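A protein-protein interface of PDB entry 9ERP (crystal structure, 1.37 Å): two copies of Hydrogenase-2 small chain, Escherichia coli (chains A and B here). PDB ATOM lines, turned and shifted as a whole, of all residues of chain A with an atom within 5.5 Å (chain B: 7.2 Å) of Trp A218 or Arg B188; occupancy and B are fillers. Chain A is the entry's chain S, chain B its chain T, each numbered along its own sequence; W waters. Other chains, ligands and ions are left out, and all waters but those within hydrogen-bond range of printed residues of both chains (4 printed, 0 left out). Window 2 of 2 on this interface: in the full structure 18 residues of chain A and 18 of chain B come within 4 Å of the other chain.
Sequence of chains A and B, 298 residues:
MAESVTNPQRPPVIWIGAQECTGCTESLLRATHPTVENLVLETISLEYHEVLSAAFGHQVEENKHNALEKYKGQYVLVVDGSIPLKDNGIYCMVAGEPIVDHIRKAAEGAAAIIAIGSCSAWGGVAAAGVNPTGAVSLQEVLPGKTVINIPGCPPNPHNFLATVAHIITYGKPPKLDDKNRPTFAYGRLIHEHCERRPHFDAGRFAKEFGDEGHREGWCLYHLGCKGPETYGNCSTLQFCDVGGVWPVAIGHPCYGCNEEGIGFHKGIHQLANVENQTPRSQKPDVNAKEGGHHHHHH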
ATOM      1  N   ARG A 196      -5.649  -6.980   1.532  1.00  0.00           N
ATOM      2  CA  ARG A 196      -6.480  -8.141   1.767  1.00  0.00           C
ATOM      3  C   ARG A 196      -6.515  -8.533   3.229  1.00  0.00           C
ATOM      4  O   ARG A 196      -7.170  -9.529   3.578  1.00  0.00           O
ATOM      5  CB  ARG A 196      -6.031  -9.311   0.888  1.00  0.00           C
ATOM      6  CG  ARG A 196      -6.086  -8.918  -0.593  1.00  0.00           C
ATOM      7  CD  ARG A 196      -6.072 -10.082  -1.542  1.00  0.00           C
ATOM      8  NE  ARG A 196      -6.184  -9.584  -2.908  1.00  0.00           N
ATOM      9  CZ  ARG A 196      -6.523 -10.327  -3.947  1.00  0.00           C
ATOM     10  NH1 ARG A 196      -6.705 -11.628  -3.825  1.00  0.00           N
ATOM     11  NH2 ARG A 196      -6.648  -9.758  -5.140  1.00  0.00           N
ATOM     12  N   HIS A 199      -9.869  -9.554   4.746  1.00  0.00           N
ATOM     13  CA  HIS A 199     -10.333 -10.898   4.439  1.00  0.00           C
ATOM     14  C   HIS A 199      -9.639 -11.924   5.322  1.00  0.00           C
ATOM     15  O   HIS A 199     -10.294 -12.828   5.848  1.00  0.00           O
ATOM     16  CB  HIS A 199     -10.094 -11.162   2.954  1.00  0.00           C
ATOM     17  CG  HIS A 199     -10.752 -10.146   2.077  1.00  0.00           C
ATOM     18  ND1 HIS A 199     -12.101  -9.873   2.138  1.00  0.00           N
ATOM     19  CD2 HIS A 199     -10.243  -9.324   1.128  1.00  0.00           C
ATOM     20  CE1 HIS A 199     -12.401  -8.930   1.265  1.00  0.00           C
ATOM     21  NE2 HIS A 199     -11.288  -8.575   0.642  1.00  0.00           N
ATOM     22  N   ARG A 204     -11.885 -15.054   5.320  1.00  0.00           N
ATOM     23  CA  ARG A 204     -12.313 -15.102   3.922  1.00  0.00           C
ATOM     24  C   ARG A 204     -11.080 -15.416   3.075  1.00  0.00           C
ATOM     25  O   ARG A 204     -10.247 -14.540   2.809  1.00  0.00           O
ATOM     26  CB  ARG A 204     -12.933 -13.766   3.517  1.00  0.00           C
ATOM     27  CG  ARG A 204     -14.380 -13.604   4.020  1.00  0.00           C
ATOM     28  CD  ARG A 204     -15.044 -12.364   3.444  1.00  0.00           C
ATOM     29  NE  ARG A 204     -14.256 -11.161   3.671  1.00  0.00           N
ATOM     30  CZ  ARG A 204     -14.574 -10.193   4.524  1.00  0.00           C
ATOM     31  NH1 ARG A 204     -15.630 -10.285   5.319  1.00  0.00           N
ATOM     32  NH2 ARG A 204     -13.820  -9.100   4.581  1.00  0.00           N
ATOM     33  N   PHE A 205     -10.952 -16.681   2.663  1.00  0.00           N
ATOM     34  CA  PHE A 205      -9.734 -17.176   2.042  1.00  0.00           C
ATOM     35  C   PHE A 205     -10.029 -17.876   0.728  1.00  0.00           C
ATOM     36  O   PHE A 205     -10.961 -18.682   0.641  1.00  0.00           O
ATOM     37  CB  PHE A 205      -9.039 -18.218   2.937  1.00  0.00           C
ATOM     38  CG  PHE A 205      -8.558 -17.700   4.270  1.00  0.00           C
ATOM     39  CD1 PHE A 205      -7.508 -16.802   4.347  1.00  0.00           C
ATOM     40  CD2 PHE A 205      -9.114 -18.165   5.459  1.00  0.00           C
ATOM     41  CE1 PHE A 205      -7.033 -16.352   5.570  1.00  0.00           C
ATOM     42  CE2 PHE A 205      -8.633 -17.735   6.675  1.00  0.00           C
ATOM     43  CZ  PHE A 205      -7.611 -16.812   6.748  1.00  0.00           C
ATOM     44  N   ALA A 206      -9.216 -17.587  -0.290  1.00  0.00           N
ATOM     45  CA  ALA A 206      -9.151 -18.456  -1.454  1.00  0.00           C
ATOM     46  C   ALA A 206      -8.562 -19.797  -1.039  1.00  0.00           C
ATOM     47  O   ALA A 206      -7.609 -19.858  -0.269  1.00  0.00           O
ATOM     48  CB  ALA A 206      -8.249 -17.829  -2.524  1.00  0.00           C
ATOM     49  N   GLY A 213     -13.894 -17.637  -3.688  1.00  0.00           N
ATOM     50  CA  GLY A 213     -13.225 -16.616  -2.903  1.00  0.00           C
ATOM     51  C   GLY A 213     -12.081 -15.967  -3.661  1.00  0.00           C
ATOM     52  O   GLY A 213     -11.886 -14.747  -3.586  1.00  0.00           O
ATOM     53  N   HIS A 214     -11.300 -16.776  -4.374  1.00  0.00           N
ATOM     54  CA  HIS A 214     -10.253 -16.235  -5.232  1.00  0.00           C
ATOM     55  C   HIS A 214     -10.827 -15.234  -6.217  1.00  0.00           C
ATOM     56  O   HIS A 214     -10.220 -14.176  -6.470  1.00  0.00           O
ATOM     57  CB  HIS A 214      -9.609 -17.401  -5.979  1.00  0.00           C
ATOM     58  CG  HIS A 214      -8.384 -17.028  -6.749  1.00  0.00           C
ATOM     59  ND1 HIS A 214      -8.276 -17.268  -8.102  1.00  0.00           N
ATOM     60  CD2 HIS A 214      -7.211 -16.476  -6.365  1.00  0.00           C
ATOM     61  CE1 HIS A 214      -7.092 -16.862  -8.524  1.00  0.00           C
ATOM     62  NE2 HIS A 214      -6.426 -16.372  -7.487  1.00  0.00           N
ATOM     63  N   GLU A 216     -13.333 -13.408  -5.819  1.00  0.00           N
ATOM     64  CA  GLU A 216     -13.781 -12.214  -5.125  1.00  0.00           C
ATOM     65  C   GLU A 216     -12.622 -11.410  -4.534  1.00  0.00           C
ATOM     66  O   GLU A 216     -12.866 -10.423  -3.838  1.00  0.00           O
ATOM     67  CB  GLU A 216     -14.796 -12.595  -4.053  1.00  0.00           C
ATOM     68  CG  GLU A 216     -16.121 -13.165  -4.600  1.00  0.00           C
ATOM     69  CD  GLU A 216     -16.835 -12.263  -5.620  1.00  0.00           C
ATOM     70  OE1 GLU A 216     -16.690 -11.011  -5.572  1.00  0.00           O
ATOM     71  OE2 GLU A 216     -17.562 -12.815  -6.480  1.00  0.00           O
ATOM     72  N   GLY A 217     -11.377 -11.793  -4.810  1.00  0.00           N
ATOM     73  CA  GLY A 217     -10.251 -11.064  -4.297  1.00  0.00           C
ATOM     74  C   GLY A 217      -9.969 -11.282  -2.840  1.00  0.00           C
ATOM     75  O   GLY A 217      -9.438 -10.385  -2.186  1.00  0.00           O
ATOM     76  N   TRP A 218     -10.274 -12.462  -2.307  1.00  0.00           N
ATOM     77  CA  TRP A 218     -10.041 -12.720  -0.898  1.00  0.00           C
ATOM     78  C   TRP A 218      -8.566 -12.988  -0.598  1.00  0.00           C
ATOM     79  O   TRP A 218      -7.698 -13.035  -1.484  1.00  0.00           O
ATOM     80  CB  TRP A 218     -10.883 -13.912  -0.459  1.00  0.00           C
ATOM     81  CG  TRP A 218     -12.338 -13.605  -0.329  1.00  0.00           C
ATOM     82  CD1 TRP A 218     -12.957 -12.413  -0.567  1.00  0.00           C
ATOM     83  CD2 TRP A 218     -13.362 -14.521   0.061  1.00  0.00           C
ATOM     84  NE1 TRP A 218     -14.310 -12.534  -0.344  1.00  0.00           N
ATOM     85  CE2 TRP A 218     -14.572 -13.827   0.036  1.00  0.00           C
ATOM     86  CE3 TRP A 218     -13.361 -15.867   0.424  1.00  0.00           C
ATOM     87  CZ2 TRP A 218     -15.794 -14.431   0.386  1.00  0.00           C
ATOM     88  CZ3 TRP A 218     -14.571 -16.469   0.774  1.00  0.00           C
ATOM     89  CH2 TRP A 218     -15.763 -15.750   0.729  1.00  0.00           C
ATOM     90  N   CYS A 219      -8.265 -13.136   0.693  1.00  0.00           N
ATOM     91  CA  CYS A 219      -6.884 -13.304   1.133  1.00  0.00           C
ATOM     92  C   CYS A 219      -6.305 -14.605   0.596  1.00  0.00           C
ATOM     93  O   CYS A 219      -7.001 -15.613   0.461  1.00  0.00           O
ATOM     94  CB  CYS A 219      -6.822 -13.277   2.664  1.00  0.00           C
ATOM     95  SG  CYS A 219      -5.276 -13.805   3.437  1.00  0.00           S
ATOM     96  N   LEU A 220      -5.012 -14.571   0.303  1.00  0.00           N
ATOM     97  CA  LEU A 220      -4.305 -15.700  -0.308  1.00  0.00           C
ATOM     98  C   LEU A 220      -3.452 -16.492   0.684  1.00  0.00           C
ATOM     99  O   LEU A 220      -2.622 -17.309   0.263  1.00  0.00           O
ATOM    100  CB  LEU A 220      -3.461 -15.213  -1.492  1.00  0.00           C
ATOM    101  CG  LEU A 220      -4.233 -14.388  -2.534  1.00  0.00           C
ATOM    102  CD1 LEU A 220      -3.309 -14.036  -3.713  1.00  0.00           C
ATOM    103  CD2 LEU A 220      -5.470 -15.077  -3.018  1.00  0.00           C
ATOM    104  N   ASP B 177     -25.642  -4.016  -7.452  1.00  0.00           N
ATOM    105  CA  ASP B 177     -26.063  -4.305  -6.092  1.00  0.00           C
ATOM    106  C   ASP B 177     -27.499  -3.798  -5.911  1.00  0.00           C
ATOM    107  O   ASP B 177     -28.164  -3.400  -6.880  1.00  0.00           O
ATOM    108  CB  ASP B 177     -25.063  -3.779  -5.055  1.00  0.00           C
ATOM    109  CG  ASP B 177     -24.983  -2.253  -5.011  1.00  0.00           C
ATOM    110  OD1 ASP B 177     -25.862  -1.595  -5.582  1.00  0.00           O
ATOM    111  OD2 ASP B 177     -24.013  -1.739  -4.374  1.00  0.00           O
ATOM    112  N   ARG B 181     -25.717  -0.125  -8.138  1.00  0.00           N
ATOM    113  CA  ARG B 181     -24.295   0.214  -8.345  1.00  0.00           C
ATOM    114  C   ARG B 181     -23.555  -0.994  -8.889  1.00  0.00           C
ATOM    115  O   ARG B 181     -23.728  -2.104  -8.363  1.00  0.00           O
ATOM    116  CB  ARG B 181     -23.652   0.634  -7.032  1.00  0.00           C
ATOM    117  CG  ARG B 181     -24.348   1.810  -6.342  1.00  0.00           C
ATOM    118  CD  ARG B 181     -23.670   2.187  -5.024  1.00  0.00           C
ATOM    119  NE  ARG B 181     -23.767   1.117  -4.034  1.00  0.00           N
ATOM    120  CZ  ARG B 181     -23.556   1.262  -2.735  1.00  0.00           C
ATOM    121  NH1 ARG B 181     -23.264   2.437  -2.210  1.00  0.00           N
ATOM    122  NH2 ARG B 181     -23.617   0.188  -1.935  1.00  0.00           N
ATOM    123  N   PRO B 182     -22.725  -0.834  -9.914  1.00  0.00           N
ATOM    124  CA  PRO B 182     -21.970  -1.987 -10.441  1.00  0.00           C
ATOM    125  C   PRO B 182     -21.080  -2.618  -9.381  1.00  0.00           C
ATOM    126  O   PRO B 182     -20.263  -1.940  -8.755  1.00  0.00           O
ATOM    127  CB  PRO B 182     -21.142  -1.365 -11.570  1.00  0.00           C
ATOM    128  CG  PRO B 182     -21.923  -0.187 -12.002  1.00  0.00           C
ATOM    129  CD  PRO B 182     -22.547   0.371 -10.747  1.00  0.00           C
ATOM    130  N   THR B 183     -21.224  -3.943  -9.205  1.00  0.00           N
ATOM    131  CA  THR B 183     -20.489  -4.627  -8.152  1.00  0.00           C
ATOM    132  C   THR B 183     -18.979  -4.595  -8.368  1.00  0.00           C
ATOM    133  O   THR B 183     -18.221  -4.662  -7.398  1.00  0.00           O
ATOM    134  CB  THR B 183     -20.952  -6.075  -7.986  1.00  0.00           C
ATOM    135  OG1 THR B 183     -20.724  -6.809  -9.188  1.00  0.00           O
ATOM    136  CG2 THR B 183     -22.437  -6.117  -7.622  1.00  0.00           C
ATOM    137  N   PHE B 184     -18.515  -4.515  -9.616  1.00  0.00           N
ATOM    138  CA  PHE B 184     -17.062  -4.516  -9.799  1.00  0.00           C
ATOM    139  C   PHE B 184     -16.411  -3.303  -9.140  1.00  0.00           C
ATOM    140  O   PHE B 184     -15.221  -3.365  -8.832  1.00  0.00           O
ATOM    141  CB  PHE B 184     -16.667  -4.608 -11.276  1.00  0.00           C
ATOM    142  CG  PHE B 184     -16.721  -3.282 -12.013  1.00  0.00           C
ATOM    143  CD1 PHE B 184     -15.613  -2.436 -12.049  1.00  0.00           C
ATOM    144  CD2 PHE B 184     -17.868  -2.884 -12.653  1.00  0.00           C
ATOM    145  CE1 PHE B 184     -15.670  -1.238 -12.714  1.00  0.00           C
ATOM    146  CE2 PHE B 184     -17.939  -1.680 -13.317  1.00  0.00           C
ATOM    147  CZ  PHE B 184     -16.839  -0.853 -13.347  1.00  0.00           C
ATOM    148  N   ALA B 185     -17.154  -2.206  -8.957  1.00  0.00           N
ATOM    149  CA  ALA B 185     -16.630  -0.969  -8.387  1.00  0.00           C
ATOM    150  C   ALA B 185     -17.157  -0.631  -7.003  1.00  0.00           C
ATOM    151  O   ALA B 185     -16.463   0.071  -6.256  1.00  0.00           O
ATOM    152  CB  ALA B 185     -16.916   0.221  -9.326  1.00  0.00           C
ATOM    153  N   TYR B 186     -18.359  -1.117  -6.644  1.00  0.00           N
ATOM    154  CA  TYR B 186     -18.995  -0.739  -5.391  1.00  0.00           C
ATOM    155  C   TYR B 186     -19.406  -1.930  -4.541  1.00  0.00           C
ATOM    156  O   TYR B 186     -20.149  -1.746  -3.575  1.00  0.00           O
ATOM    157  CB  TYR B 186     -20.186   0.182  -5.656  1.00  0.00           C
ATOM    158  CG  TYR B 186     -19.785   1.379  -6.481  1.00  0.00           C
ATOM    159  CD1 TYR B 186     -19.247   2.514  -5.878  1.00  0.00           C
ATOM    160  CD2 TYR B 186     -19.908   1.363  -7.864  1.00  0.00           C
ATOM    161  CE1 TYR B 186     -18.849   3.604  -6.639  1.00  0.00           C
ATOM    162  CE2 TYR B 186     -19.526   2.454  -8.637  1.00  0.00           C
ATOM    163  CZ  TYR B 186     -18.988   3.576  -8.011  1.00  0.00           C
ATOM    164  OH  TYR B 186     -18.583   4.652  -8.760  1.00  0.00           O
ATOM    165  N   GLY B 187     -18.935  -3.115  -4.847  1.00  0.00           N
ATOM    166  CA  GLY B 187     -19.384  -4.313  -4.171  1.00  0.00           C
ATOM    167  C   GLY B 187     -18.882  -4.555  -2.771  1.00  0.00           C
ATOM    168  O   GLY B 187     -19.328  -5.517  -2.135  1.00  0.00           O
ATOM    169  N   ARG B 188     -17.974  -3.732  -2.254  1.00  0.00           N
ATOM    170  CA  ARG B 188     -17.283  -4.001  -1.000  1.00  0.00           C
ATOM    171  C   ARG B 188     -17.026  -2.683  -0.283  1.00  0.00           C
ATOM    172  O   ARG B 188     -16.754  -1.666  -0.933  1.00  0.00           O
ATOM    173  CB  ARG B 188     -15.903  -4.666  -1.300  1.00  0.00           C
ATOM    174  CG  ARG B 188     -15.052  -5.041  -0.099  1.00  0.00           C
ATOM    175  CD  ARG B 188     -14.000  -6.095  -0.474  1.00  0.00           C
ATOM    176  NE  ARG B 188     -14.626  -7.332  -0.925  1.00  0.00           N
ATOM    177  CZ  ARG B 188     -14.072  -8.187  -1.777  1.00  0.00           C
ATOM    178  NH1 ARG B 188     -12.894  -7.948  -2.323  1.00  0.00           N
ATOM    179  NH2 ARG B 188     -14.723  -9.307  -2.089  1.00  0.00           N
ATOM    180  N   LEU B 189     -17.071  -2.714   1.055  1.00  0.00           N
ATOM    181  CA  LEU B 189     -16.646  -1.569   1.844  1.00  0.00           C
ATOM    182  C   LEU B 189     -15.161  -1.281   1.619  1.00  0.00           C
ATOM    183  O   LEU B 189     -14.319  -2.180   1.519  1.00  0.00           O
ATOM    184  CB  LEU B 189     -16.863  -1.839   3.338  1.00  0.00           C
ATOM    185  CG  LEU B 189     -18.318  -1.885   3.801  1.00  0.00           C
ATOM    186  CD1 LEU B 189     -18.357  -2.488   5.213  1.00  0.00           C
ATOM    187  CD2 LEU B 189     -18.966  -0.504   3.751  1.00  0.00           C
ATOM    188  N   ILE B 190     -14.813  -0.006   1.605  1.00  0.00           N
ATOM    189  CA  ILE B 190     -13.399   0.336   1.482  1.00  0.00           C
ATOM    190  C   ILE B 190     -12.578  -0.276   2.614  1.00  0.00           C
ATOM    191  O   ILE B 190     -11.500  -0.833   2.389  1.00  0.00           O
ATOM    192  CB  ILE B 190     -13.242   1.871   1.394  1.00  0.00           C
ATOM    193  CG1 ILE B 190     -13.799   2.348   0.047  1.00  0.00           C
ATOM    194  CG2 ILE B 190     -11.801   2.280   1.605  1.00  0.00           C
ATOM    195  CD1 ILE B 190     -13.955   3.893  -0.039  1.00  0.00           C
ATOM    196  N   HIS B 191     -13.103  -0.230   3.842  1.00  0.00           N
ATOM    197  CA  HIS B 191     -12.423  -0.776   5.007  1.00  0.00           C
ATOM    198  C   HIS B 191     -12.270  -2.289   4.939  1.00  0.00           C
ATOM    199  O   HIS B 191     -11.407  -2.825   5.641  1.00  0.00           O
ATOM    200  CB  HIS B 191     -13.259  -0.375   6.219  1.00  0.00           C
ATOM    201  CG  HIS B 191     -12.723  -0.814   7.542  1.00  0.00           C
ATOM    202  ND1 HIS B 191     -11.627  -0.233   8.143  1.00  0.00           N
ATOM    203  CD2 HIS B 191     -13.185  -1.745   8.416  1.00  0.00           C
ATOM    204  CE1 HIS B 191     -11.422  -0.806   9.314  1.00  0.00           C
ATOM    205  NE2 HIS B 191     -12.359  -1.719   9.502  1.00  0.00           N
ATOM    206  N   GLU B 192     -13.069  -2.973   4.132  1.00  0.00           N
ATOM    207  CA  GLU B 192     -12.928  -4.417   3.950  1.00  0.00           C
ATOM    208  C   GLU B 192     -11.991  -4.764   2.811  1.00  0.00           C
ATOM    209  O   GLU B 192     -11.912  -5.942   2.423  1.00  0.00           O
ATOM    210  CB  GLU B 192     -14.295  -5.077   3.768  1.00  0.00           C
ATOM    211  CG  GLU B 192     -15.139  -5.008   5.037  1.00  0.00           C
ATOM    212  CD  GLU B 192     -14.455  -5.674   6.215  1.00  0.00           C
ATOM    213  OE1 GLU B 192     -14.021  -6.837   6.077  1.00  0.00           O
ATOM    214  OE2 GLU B 192     -14.304  -5.028   7.283  1.00  0.00           O
ATOM    215  N   HIS B 193     -11.262  -3.764   2.281  1.00  0.00           N
ATOM    216  CA  HIS B 193     -10.200  -4.026   1.304  1.00  0.00           C
ATOM    217  C   HIS B 193      -9.168  -2.893   1.341  1.00  0.00           C
ATOM    218  O   HIS B 193      -8.655  -2.451   0.303  1.00  0.00           O
ATOM    219  CB  HIS B 193     -10.768  -4.244  -0.102  1.00  0.00           C
ATOM    220  CG  HIS B 193      -9.961  -5.185  -0.935  1.00  0.00           C
ATOM    221  ND1 HIS B 193     -10.417  -6.436  -1.312  1.00  0.00           N
ATOM    222  CD2 HIS B 193      -8.718  -5.065  -1.450  1.00  0.00           C
ATOM    223  CE1 HIS B 193      -9.476  -7.045  -2.020  1.00  0.00           C
ATOM    224  NE2 HIS B 193      -8.438  -6.236  -2.117  1.00  0.00           N
ATOM    225  N   CYS B 194      -8.831  -2.430   2.541  1.00  0.00           N
ATOM    226  CA  CYS B 194      -7.929  -1.298   2.744  1.00  0.00           C
ATOM    227  C   CYS B 194      -6.580  -1.764   3.266  1.00  0.00           C
ATOM    228  O   CYS B 194      -6.508  -2.506   4.260  1.00  0.00           O
ATOM    229  CB  CYS B 194      -8.525  -0.325   3.765  1.00  0.00           C
ATOM    230  SG  CYS B 194      -7.411   1.052   4.085  1.00  0.00           S
ATOM    231  N   GLY B 227     -14.060   4.931   5.590  1.00  0.00           N
ATOM    232  CA  GLY B 227     -13.932   3.641   4.935  1.00  0.00           C
ATOM    233  C   GLY B 227     -14.822   2.559   5.506  1.00  0.00           C
ATOM    234  O   GLY B 227     -15.372   1.747   4.743  1.00  0.00           O
ATOM    235  N   THR B 230     -18.425   3.083   3.776  1.00  0.00           N
ATOM    236  CA  THR B 230     -18.476   3.560   2.401  1.00  0.00           C
ATOM    237  C   THR B 230     -18.122   2.426   1.461  1.00  0.00           C
ATOM    238  O   THR B 230     -17.031   1.854   1.565  1.00  0.00           O
ATOM    239  CB  THR B 230     -17.483   4.726   2.219  1.00  0.00           C
ATOM    240  OG1 THR B 230     -17.767   5.746   3.191  1.00  0.00           O
ATOM    241  CG2 THR B 230     -17.558   5.299   0.829  1.00  0.00           C
ATOM    242  N   TYR B 231     -19.042   2.112   0.547  1.00  0.00           N
ATOM    243  CA  TYR B 231     -18.771   1.141  -0.513  1.00  0.00           C
ATOM    244  C   TYR B 231     -18.038   1.821  -1.661  1.00  0.00           C
ATOM    245  O   TYR B 231     -18.424   2.906  -2.092  1.00  0.00           O
ATOM    246  CB  TYR B 231     -20.085   0.548  -1.032  1.00  0.00           C
ATOM    247  CG  TYR B 231     -20.681  -0.408  -0.036  1.00  0.00           C
ATOM    248  CD1 TYR B 231     -21.507   0.037   0.980  1.00  0.00           C
ATOM    249  CD2 TYR B 231     -20.379  -1.747  -0.096  1.00  0.00           C
ATOM    250  CE1 TYR B 231     -22.006  -0.835   1.928  1.00  0.00           C
ATOM    251  CE2 TYR B 231     -20.887  -2.636   0.840  1.00  0.00           C
ATOM    252  CZ  TYR B 231     -21.716  -2.167   1.837  1.00  0.00           C
ATOM    253  OH  TYR B 231     -22.210  -3.067   2.769  1.00  0.00           O
ATOM    254  N   GLY B 232     -17.026   1.144  -2.196  1.00  0.00           N
ATOM    255  CA  GLY B 232     -16.255   1.723  -3.276  1.00  0.00           C
ATOM    256  C   GLY B 232     -15.035   0.888  -3.599  1.00  0.00           C
ATOM    257  O   GLY B 232     -14.744  -0.135  -2.960  1.00  0.00           O
ATOM    258  N   ASN B 233     -14.308   1.350  -4.628  1.00  0.00           N
ATOM    259  CA  ASN B 233     -13.066   0.695  -5.043  1.00  0.00           C
ATOM    260  C   ASN B 233     -11.857   1.621  -4.915  1.00  0.00           C
ATOM    261  O   ASN B 233     -10.832   1.419  -5.562  1.00  0.00           O
ATOM    262  CB  ASN B 233     -13.215   0.131  -6.448  1.00  0.00           C
ATOM    263  CG  ASN B 233     -13.414   1.198  -7.506  1.00  0.00           C
ATOM    264  OD1 ASN B 233     -13.486   2.390  -7.213  1.00  0.00           O
ATOM    265  ND2 ASN B 233     -13.557   0.769  -8.740  1.00  0.00           N
ATOM    266  N   CYS B 234     -11.931   2.592  -4.007  1.00  0.00           N
ATOM    267  CA  CYS B 234     -10.881   3.611  -3.945  1.00  0.00           C
ATOM    268  C   CYS B 234      -9.539   3.053  -3.505  1.00  0.00           C
ATOM    269  O   CYS B 234      -8.505   3.578  -3.913  1.00  0.00           O
ATOM    270  CB  CYS B 234     -11.312   4.740  -3.019  1.00  0.00           C
ATOM    271  SG  CYS B 234     -12.843   5.495  -3.568  1.00  0.00           S
ATOM    272  N   THR B 236      -8.385   0.015  -4.194  1.00  0.00           N
ATOM    273  CA  THR B 236      -7.867  -0.960  -5.156  1.00  0.00           C
ATOM    274  C   THR B 236      -7.645  -0.278  -6.502  1.00  0.00           C
ATOM    275  O   THR B 236      -6.486  -0.108  -6.939  1.00  0.00           O
ATOM    276  CB  THR B 236      -8.759  -2.200  -5.288  1.00  0.00           C
ATOM    277  OG1 THR B 236     -10.129  -1.819  -5.454  1.00  0.00           O
ATOM    278  CG2 THR B 236      -8.643  -3.125  -4.075  1.00  0.00           C
HETATM  279  O   HOH W   1     -16.957  -8.170   7.099  1.00  0.00           O
HETATM  280  O   HOH W   2     -15.076  -8.819  -5.507  1.00  0.00           O
HETATM  281  O   HOH W   3     -16.914 -11.160  -0.700  1.00  0.00           O
HETATM  282  O   HOH W   4      -6.018  -6.731  -3.720  1.00  0.00           O
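Of the printed residues of chain B, Arg A196 touches His B193. Of the printed residues of chain B, His A199 touches Arg B188 (3.4 Å), Glu B192 (3.2 Å) and His B193 (3.0 Å). Printed residues of chain B within 4 Å of Arg A204: Glu B192. Of the printed residues of chain B, Trp A218 touches Arg B188. Arg B188 touches just these residues of chain A: His A199, Glu A216 and Trp A218. Of the printed residues of chain A, Glu B192 touches His A199 and Arg A204. Printed residues of chain A within 4 Å of His B193: Arg A196, His A199 and Gly A217. The nearest residue of chain B that does not touch Trp A218 is His B193 (5.5 Å).
Among the printed residues, 8 pairs touch across the chains.
The guanidinium group (NH1) of Arg B188 sits at hydrogen-bond distance from a ring nitrogen (NE2) of His A199 (3.4 Å). ND1 of His B193 is in hydrogen-bond range of NE2 of His A199, 3.0 Å away. NE2 of His A199 sits at hydrogen-bond distance from O of Glu B192 (3.2 Å). The backbone carbonyl oxygen (O) of Glu A216 is in hydrogen-bond range of the guanidinium group (NH2) of Arg B188, at 2.8 Å. The guanidinium group of Arg A204 lies within salt-bridge range of the side-chain carboxylate of Glu B192 (2.7 Å).
No position is printed for both chains. Of the 8 pairs that touch across the chains among the printed residues, none has its exchanged pair printed and touching as well.
Water W2 bridges the side-chain carboxylate (OE1) of Glu A216 (2.7 Å) and the guanidinium group (NH2) of Arg B188 (3.5 Å). Water W4 bridges a ring nitrogen (NE2) of His B193 (2.9 Å) and the guanidinium group of Arg A196 (3.0 Å). Water W3 lies within hydrogen-bond range of NE1 of Trp A218 (3.0 Å) and NH2 of Arg B188 (3.2 Å). Water W1 lies within hydrogen-bond range of the guanidinium group of Arg A204 and the side-chain carboxylate of Glu B192.
NE2 of His B193 touches CG of Arg A196, 3.9 Å away. CE1 of His B193 touches O of Gly A217 (3.3 Å). NE1 of Trp A218 touches NH2 of Arg B188, 3.7 Å away.
The backbone carbonyl oxygen (O) of Gly A213 lies within hydrogen-bond range of the backbone NH (N) of Trp A218, at 3.1 Å. O of Arg A204 is in hydrogen-bond range of N of Cys A219. The backbone carbonyl oxygen (O) of His A199 sits at hydrogen-bond distance from the backbone NH (N) of Arg A204, 2.8 Å away. The guanidinium group (NH1) of Arg A196 lies close to the backbone carbonyl oxygen (O) of Gly A217 (3.4 Å). The guanidinium group (NH1) of Arg A196 is in hydrogen-bond range of the backbone carbonyl oxygen (O) of Trp A218, at 2.9 Å. ND1 of His B193 lies within hydrogen-bond range of NH1 of Arg B188 (3.1 Å).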
